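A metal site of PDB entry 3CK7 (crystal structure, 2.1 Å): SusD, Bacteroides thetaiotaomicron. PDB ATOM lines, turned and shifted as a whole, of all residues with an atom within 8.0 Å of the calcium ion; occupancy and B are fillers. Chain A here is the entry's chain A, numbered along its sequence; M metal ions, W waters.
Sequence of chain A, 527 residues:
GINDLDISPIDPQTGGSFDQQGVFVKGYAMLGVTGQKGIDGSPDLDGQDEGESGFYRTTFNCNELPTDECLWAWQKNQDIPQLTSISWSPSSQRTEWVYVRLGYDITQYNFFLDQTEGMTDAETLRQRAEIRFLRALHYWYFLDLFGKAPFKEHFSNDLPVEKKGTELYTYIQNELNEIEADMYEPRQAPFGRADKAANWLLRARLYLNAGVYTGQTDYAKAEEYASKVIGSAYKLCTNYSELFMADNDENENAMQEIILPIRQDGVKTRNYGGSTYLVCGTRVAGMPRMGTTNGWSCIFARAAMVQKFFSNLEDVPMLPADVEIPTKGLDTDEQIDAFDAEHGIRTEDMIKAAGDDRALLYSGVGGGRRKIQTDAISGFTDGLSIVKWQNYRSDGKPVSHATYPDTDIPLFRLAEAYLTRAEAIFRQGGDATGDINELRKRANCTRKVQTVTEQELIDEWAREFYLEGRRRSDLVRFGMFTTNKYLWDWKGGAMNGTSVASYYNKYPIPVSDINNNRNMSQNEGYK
The side-chain carboxylate (OD2) of Asp 408 is in salt-bridge range of the guanidinium group (NE) of Arg 263. O of Asp 408 lies within hydrogen-bond range of ND2 of Asn 248. N of Gly 266 lies within hydrogen-bond range of OD1 of Asp 406. OG of Ser 400 lies within hydrogen-bond range of OD1 of Asp 406. N of Asp 406 lies close to ND2 of Asn 391 (2.9 Å). The side-chain amide oxygen (OE1) of Gln 264 is in hydrogen-bond range of the backbone NH (N) of Ser 275 (2.9 Å). OD2 of Asp 249 lies close to NH2 of Arg 263, at 3.4 Å.
Within 4 Å of the calcium ion: Asp 249, Gln 264, Asp 406 and Asp 408.
The calcium ion is bound by OD1 of Asp 408, O of Asp 406, O of Gln 264, water W1, OD2 of Asp 249, water W2 and water W3. The calcium ion has seven donor atoms within binding distance.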
ATOM      1  N   PHE A 191       4.596 -29.879   4.193  1.00  0.00           N
ATOM      2  CA  PHE A 191       4.511 -28.561   3.570  1.00  0.00           C
ATOM      3  C   PHE A 191       5.457 -28.427   2.382  1.00  0.00           C
ATOM      4  O   PHE A 191       6.668 -28.578   2.512  1.00  0.00           O
ATOM      5  CB  PHE A 191       4.812 -27.450   4.585  1.00  0.00           C
ATOM      6  CG  PHE A 191       4.469 -26.069   4.077  1.00  0.00           C
ATOM      7  CD1 PHE A 191       3.141 -25.720   3.855  1.00  0.00           C
ATOM      8  CD2 PHE A 191       5.471 -25.149   3.780  1.00  0.00           C
ATOM      9  CE1 PHE A 191       2.808 -24.464   3.331  1.00  0.00           C
ATOM     10  CE2 PHE A 191       5.148 -23.891   3.256  1.00  0.00           C
ATOM     11  CZ  PHE A 191       3.823 -23.550   3.037  1.00  0.00           C
ATOM     12  N   MET A 245       4.583 -12.788   3.312  1.00  0.00           N
ATOM     13  CA  MET A 245       5.673 -12.416   4.213  1.00  0.00           C
ATOM     14  C   MET A 245       6.720 -13.512   4.364  1.00  0.00           C
ATOM     15  O   MET A 245       6.472 -14.684   4.060  1.00  0.00           O
ATOM     16  CB  MET A 245       5.107 -12.012   5.577  1.00  0.00           C
ATOM     17  CG  MET A 245       4.386 -10.672   5.540  1.00  0.00           C
ATOM     18  SD  MET A 245       3.847 -10.117   7.158  1.00  0.00           S
ATOM     19  CE  MET A 245       2.689  -8.888   6.716  1.00  0.00           C
ATOM     20  N   ALA A 246       7.885 -13.118   4.842  1.00  0.00           N
ATOM     21  CA  ALA A 246       9.028 -14.017   5.008  1.00  0.00           C
ATOM     22  C   ALA A 246       8.780 -15.283   5.821  1.00  0.00           C
ATOM     23  O   ALA A 246       9.481 -16.266   5.626  1.00  0.00           O
ATOM     24  CB  ALA A 246      10.203 -13.228   5.582  1.00  0.00           C
ATOM     25  N   ASP A 247       7.813 -15.269   6.728  1.00  0.00           N
ATOM     26  CA  ASP A 247       7.556 -16.462   7.535  1.00  0.00           C
ATOM     27  C   ASP A 247       6.282 -17.187   7.135  1.00  0.00           C
ATOM     28  O   ASP A 247       5.687 -17.895   7.947  1.00  0.00           O
ATOM     29  CB  ASP A 247       7.513 -16.101   9.023  1.00  0.00           C
ATOM     30  CG  ASP A 247       6.368 -15.169   9.369  1.00  0.00           C
ATOM     31  OD1 ASP A 247       5.930 -14.389   8.497  1.00  0.00           O
ATOM     32  OD2 ASP A 247       5.912 -15.200  10.539  1.00  0.00           O
ATOM     33  N   ASN A 248       5.859 -17.043   5.874  1.00  0.00           N
ATOM     34  CA  ASN A 248       4.639 -17.703   5.431  1.00  0.00           C
ATOM     35  C   ASN A 248       4.749 -19.218   5.391  1.00  0.00           C
ATOM     36  O   ASN A 248       3.760 -19.901   5.126  1.00  0.00           O
ATOM     37  CB  ASN A 248       4.174 -17.166   4.072  1.00  0.00           C
ATOM     38  CG  ASN A 248       5.231 -17.247   2.991  1.00  0.00           C
ATOM     39  OD1 ASN A 248       6.320 -17.752   3.208  1.00  0.00           O
ATOM     40  ND2 ASN A 248       4.900 -16.754   1.793  1.00  0.00           N
ATOM     41  N   ASP A 249       5.930 -19.757   5.657  1.00  0.00           N
ATOM     42  CA  ASP A 249       6.110 -21.209   5.671  1.00  0.00           C
ATOM     43  C   ASP A 249       6.102 -21.740   7.093  1.00  0.00           C
ATOM     44  O   ASP A 249       6.180 -22.948   7.320  1.00  0.00           O
ATOM     45  CB  ASP A 249       7.398 -21.637   4.957  1.00  0.00           C
ATOM     46  CG  ASP A 249       8.633 -20.968   5.526  1.00  0.00           C
ATOM     47  OD1 ASP A 249       8.574 -20.414   6.640  1.00  0.00           O
ATOM     48  OD2 ASP A 249       9.683 -21.014   4.849  1.00  0.00           O
ATOM     49  N   GLU A 250       6.008 -20.832   8.061  1.00  0.00           N
ATOM     50  CA  GLU A 250       5.984 -21.177   9.486  1.00  0.00           C
ATOM     51  C   GLU A 250       4.760 -20.596  10.177  1.00  0.00           C
ATOM     52  O   GLU A 250       4.352 -21.094  11.227  1.00  0.00           O
ATOM     53  CB  GLU A 250       7.221 -20.648  10.205  1.00  0.00           C
ATOM     54  CG  GLU A 250       8.505 -21.378   9.938  1.00  0.00           C
ATOM     55  CD  GLU A 250       9.670 -20.730  10.641  1.00  0.00           C
ATOM     56  OE1 GLU A 250       9.566 -20.468  11.864  1.00  0.00           O
ATOM     57  OE2 GLU A 250      10.699 -20.484   9.991  1.00  0.00           O
ATOM     58  N   ILE A 262       5.958 -22.493  -3.292  1.00  0.00           N
ATOM     59  CA  ILE A 262       7.219 -22.689  -3.988  1.00  0.00           C
ATOM     60  C   ILE A 262       8.187 -22.203  -2.911  1.00  0.00           C
ATOM     61  O   ILE A 262       8.253 -21.005  -2.614  1.00  0.00           O
ATOM     62  CB  ILE A 262       7.370 -21.785  -5.235  1.00  0.00           C
ATOM     63  CG1 ILE A 262       6.362 -22.189  -6.302  1.00  0.00           C
ATOM     64  CG2 ILE A 262       8.802 -21.886  -5.779  1.00  0.00           C
ATOM     65  CD1 ILE A 262       6.422 -21.335  -7.556  1.00  0.00           C
ATOM     66  N   ARG A 263       8.899 -23.143  -2.298  1.00  0.00           N
ATOM     67  CA  ARG A 263       9.831 -22.803  -1.231  1.00  0.00           C
ATOM     68  C   ARG A 263      10.975 -21.906  -1.684  1.00  0.00           C
ATOM     69  O   ARG A 263      11.541 -22.084  -2.759  1.00  0.00           O
ATOM     70  CB  ARG A 263      10.383 -24.090  -0.600  1.00  0.00           C
ATOM     71  CG  ARG A 263       9.310 -25.127  -0.241  1.00  0.00           C
ATOM     72  CD  ARG A 263       8.217 -24.535   0.644  1.00  0.00           C
ATOM     73  NE  ARG A 263       8.746 -24.067   1.923  1.00  0.00           N
ATOM     74  CZ  ARG A 263       9.164 -24.867   2.899  1.00  0.00           C
ATOM     75  NH1 ARG A 263       9.114 -26.179   2.753  1.00  0.00           N
ATOM     76  NH2 ARG A 263       9.648 -24.338   4.024  1.00  0.00           N
ATOM     77  N   GLN A 264      11.288 -20.920  -0.857  1.00  0.00           N
ATOM     78  CA  GLN A 264      12.369 -19.979  -1.127  1.00  0.00           C
ATOM     79  C   GLN A 264      13.082 -19.789   0.191  1.00  0.00           C
ATOM     80  O   GLN A 264      12.482 -19.968   1.251  1.00  0.00           O
ATOM     81  CB  GLN A 264      11.800 -18.641  -1.617  1.00  0.00           C
ATOM     82  CG  GLN A 264      11.081 -18.729  -2.953  1.00  0.00           C
ATOM     83  CD  GLN A 264      12.037 -18.839  -4.123  1.00  0.00           C
ATOM     84  OE1 GLN A 264      12.519 -17.824  -4.638  1.00  0.00           O
ATOM     85  NE2 GLN A 264      12.335 -20.070  -4.531  1.00  0.00           N
ATOM     86  N   ASP A 265      14.355 -19.439   0.144  1.00  0.00           N
ATOM     87  CA  ASP A 265      15.120 -19.226   1.371  1.00  0.00           C
ATOM     88  C   ASP A 265      16.286 -18.296   1.098  1.00  0.00           C
ATOM     89  O   ASP A 265      17.042 -18.503   0.160  1.00  0.00           O
ATOM     90  CB  ASP A 265      15.619 -20.563   1.911  1.00  0.00           C
ATOM     91  CG  ASP A 265      16.400 -20.400   3.199  1.00  0.00           C
ATOM     92  OD1 ASP A 265      17.616 -20.160   3.138  1.00  0.00           O
ATOM     93  OD2 ASP A 265      15.782 -20.511   4.275  1.00  0.00           O
ATOM     94  N   GLY A 266      16.401 -17.262   1.931  1.00  0.00           N
ATOM     95  CA  GLY A 266      17.456 -16.278   1.762  1.00  0.00           C
ATOM     96  C   GLY A 266      18.862 -16.825   1.537  1.00  0.00           C
ATOM     97  O   GLY A 266      19.604 -16.297   0.704  1.00  0.00           O
ATOM     98  N   LYS A 268      19.701 -20.605   1.405  1.00  0.00           N
ATOM     99  CA  LYS A 268      19.703 -21.844   0.645  1.00  0.00           C
ATOM    100  C   LYS A 268      19.035 -21.855  -0.729  1.00  0.00           C
ATOM    101  O   LYS A 268      19.652 -22.258  -1.705  1.00  0.00           O
ATOM    102  CB  LYS A 268      19.102 -22.973   1.488  1.00  0.00           C
ATOM    103  CG  LYS A 268      19.954 -23.357   2.687  1.00  0.00           C
ATOM    104  CD  LYS A 268      19.329 -24.476   3.515  1.00  0.00           C
ATOM    105  CE  LYS A 268      18.106 -24.006   4.291  1.00  0.00           C
ATOM    106  NZ  LYS A 268      16.990 -23.575   3.394  1.00  0.00           N
ATOM    107  N   THR A 269      17.780 -21.434  -0.792  1.00  0.00           N
ATOM    108  CA  THR A 269      17.061 -21.431  -2.066  1.00  0.00           C
ATOM    109  C   THR A 269      16.982 -20.057  -2.689  1.00  0.00           C
ATOM    110  O   THR A 269      16.024 -19.313  -2.445  1.00  0.00           O
ATOM    111  CB  THR A 269      15.642 -21.989  -1.882  1.00  0.00           C
ATOM    112  OG1 THR A 269      15.705 -23.254  -1.227  1.00  0.00           O
ATOM    113  CG2 THR A 269      14.963 -22.165  -3.247  1.00  0.00           C
ATOM    114  N   SER A 275      11.243 -15.274  -5.331  1.00  0.00           N
ATOM    115  CA  SER A 275      10.678 -14.207  -4.508  1.00  0.00           C
ATOM    116  C   SER A 275      11.637 -13.012  -4.526  1.00  0.00           C
ATOM    117  O   SER A 275      11.243 -11.879  -4.245  1.00  0.00           O
ATOM    118  CB  SER A 275      10.431 -14.690  -3.082  1.00  0.00           C
ATOM    119  OG  SER A 275      11.599 -15.232  -2.505  1.00  0.00           O
ATOM    120  N   ASN A 391       9.938  -8.994   2.718  1.00  0.00           N
ATOM    121  CA  ASN A 391      10.900  -9.908   3.310  1.00  0.00           C
ATOM    122  C   ASN A 391      10.983  -9.674   4.809  1.00  0.00           C
ATOM    123  O   ASN A 391      12.064  -9.504   5.369  1.00  0.00           O
ATOM    124  CB  ASN A 391      12.296  -9.752   2.711  1.00  0.00           C
ATOM    125  CG  ASN A 391      13.247 -10.857   3.161  1.00  0.00           C
ATOM    126  OD1 ASN A 391      14.448 -10.627   3.339  1.00  0.00           O
ATOM    127  ND2 ASN A 391      12.710 -12.050   3.345  1.00  0.00           N
ATOM    128  N   ARG A 393       9.168 -11.107   8.575  1.00  0.00           N
ATOM    129  CA  ARG A 393       8.348 -12.154   9.185  1.00  0.00           C
ATOM    130  C   ARG A 393       7.219 -11.519   9.977  1.00  0.00           C
ATOM    131  O   ARG A 393       7.395 -10.454  10.564  1.00  0.00           O
ATOM    132  CB  ARG A 393       9.203 -13.019  10.118  1.00  0.00           C
ATOM    133  CG  ARG A 393      10.280 -13.835   9.436  1.00  0.00           C
ATOM    134  CD  ARG A 393      11.126 -14.557  10.485  1.00  0.00           C
ATOM    135  NE  ARG A 393      10.338 -15.425  11.360  1.00  0.00           N
ATOM    136  CZ  ARG A 393      10.160 -16.728  11.184  1.00  0.00           C
ATOM    137  NH1 ARG A 393      10.725 -17.343  10.157  1.00  0.00           N
ATOM    138  NH2 ARG A 393       9.432 -17.432  12.042  1.00  0.00           N
ATOM    139  N   SER A 400      16.642 -14.939   7.353  1.00  0.00           N
ATOM    140  CA  SER A 400      17.958 -15.541   7.135  1.00  0.00           C
ATOM    141  C   SER A 400      19.000 -14.708   6.391  1.00  0.00           C
ATOM    142  O   SER A 400      20.198 -14.861   6.640  1.00  0.00           O
ATOM    143  CB  SER A 400      17.801 -16.878   6.406  1.00  0.00           C
ATOM    144  OG  SER A 400      17.647 -16.682   5.007  1.00  0.00           O
ATOM    145  N   PRO A 405      15.265 -12.749  -0.070  1.00  0.00           N
ATOM    146  CA  PRO A 405      14.145 -13.031   0.835  1.00  0.00           C
ATOM    147  C   PRO A 405      13.910 -14.487   1.186  1.00  0.00           C
ATOM    148  O   PRO A 405      14.294 -15.393   0.445  1.00  0.00           O
ATOM    149  CB  PRO A 405      12.950 -12.415   0.100  1.00  0.00           C
ATOM    150  CG  PRO A 405      13.298 -12.703  -1.328  1.00  0.00           C
ATOM    151  CD  PRO A 405      14.778 -12.364  -1.405  1.00  0.00           C
ATOM    152  N   ASP A 406      13.263 -14.711   2.336  1.00  0.00           N
ATOM    153  CA  ASP A 406      12.925 -16.067   2.784  1.00  0.00           C
ATOM    154  C   ASP A 406      11.522 -16.385   2.267  1.00  0.00           C
ATOM    155  O   ASP A 406      11.129 -17.561   2.141  1.00  0.00           O
ATOM    156  CB  ASP A 406      12.903 -16.146   4.323  1.00  0.00           C
ATOM    157  CG  ASP A 406      14.286 -16.181   4.941  1.00  0.00           C
ATOM    158  OD1 ASP A 406      15.296 -16.289   4.190  1.00  0.00           O
ATOM    159  OD2 ASP A 406      14.367 -16.115   6.183  1.00  0.00           O
ATOM    160  N   THR A 407      10.767 -15.328   1.983  1.00  0.00           N
ATOM    161  CA  THR A 407       9.395 -15.431   1.514  1.00  0.00           C
ATOM    162  C   THR A 407       9.136 -16.478   0.434  1.00  0.00           C
ATOM    163  O   THR A 407       9.780 -16.470  -0.612  1.00  0.00           O
ATOM    164  CB  THR A 407       8.903 -14.083   0.969  1.00  0.00           C
ATOM    165  OG1 THR A 407       9.238 -13.042   1.894  1.00  0.00           O
ATOM    166  CG2 THR A 407       7.404 -14.115   0.768  1.00  0.00           C
ATOM    167  N   ASP A 408       8.199 -17.373   0.724  1.00  0.00           N
ATOM    168  CA  ASP A 408       7.802 -18.417  -0.223  1.00  0.00           C
ATOM    169  C   ASP A 408       6.782 -17.805  -1.175  1.00  0.00           C
ATOM    170  O   ASP A 408       6.163 -16.792  -0.847  1.00  0.00           O
ATOM    171  CB  ASP A 408       7.114 -19.597   0.496  1.00  0.00           C
ATOM    172  CG  ASP A 408       8.102 -20.557   1.149  1.00  0.00           C
ATOM    173  OD1 ASP A 408       9.292 -20.210   1.293  1.00  0.00           O
ATOM    174  OD2 ASP A 408       7.665 -21.657   1.528  1.00  0.00           O
ATOM    175  N   ILE A 409       6.631 -18.395  -2.349  1.00  0.00           N
ATOM    176  CA  ILE A 409       5.655 -17.921  -3.320  1.00  0.00           C
ATOM    177  C   ILE A 409       4.447 -18.835  -3.173  1.00  0.00           C
ATOM    178  O   ILE A 409       4.513 -20.027  -3.488  1.00  0.00           O
ATOM    179  CB  ILE A 409       6.192 -18.022  -4.768  1.00  0.00           C
ATOM    180  CG1 ILE A 409       7.318 -17.001  -4.980  1.00  0.00           C
ATOM    181  CG2 ILE A 409       5.061 -17.798  -5.758  1.00  0.00           C
ATOM    182  CD1 ILE A 409       7.942 -17.064  -6.365  1.00  0.00           C
HETATM  183 CA    CA M   1      10.786 -19.770   2.934  1.00  0.00          CA
HETATM  184  O   HOH W   1      12.568 -19.464   4.682  1.00  0.00           O
HETATM  185  O   HOH W   2       8.763 -18.642   3.993  1.00  0.00           O
HETATM  186  O   HOH W   3      11.968 -22.196   2.623  1.00  0.00           O
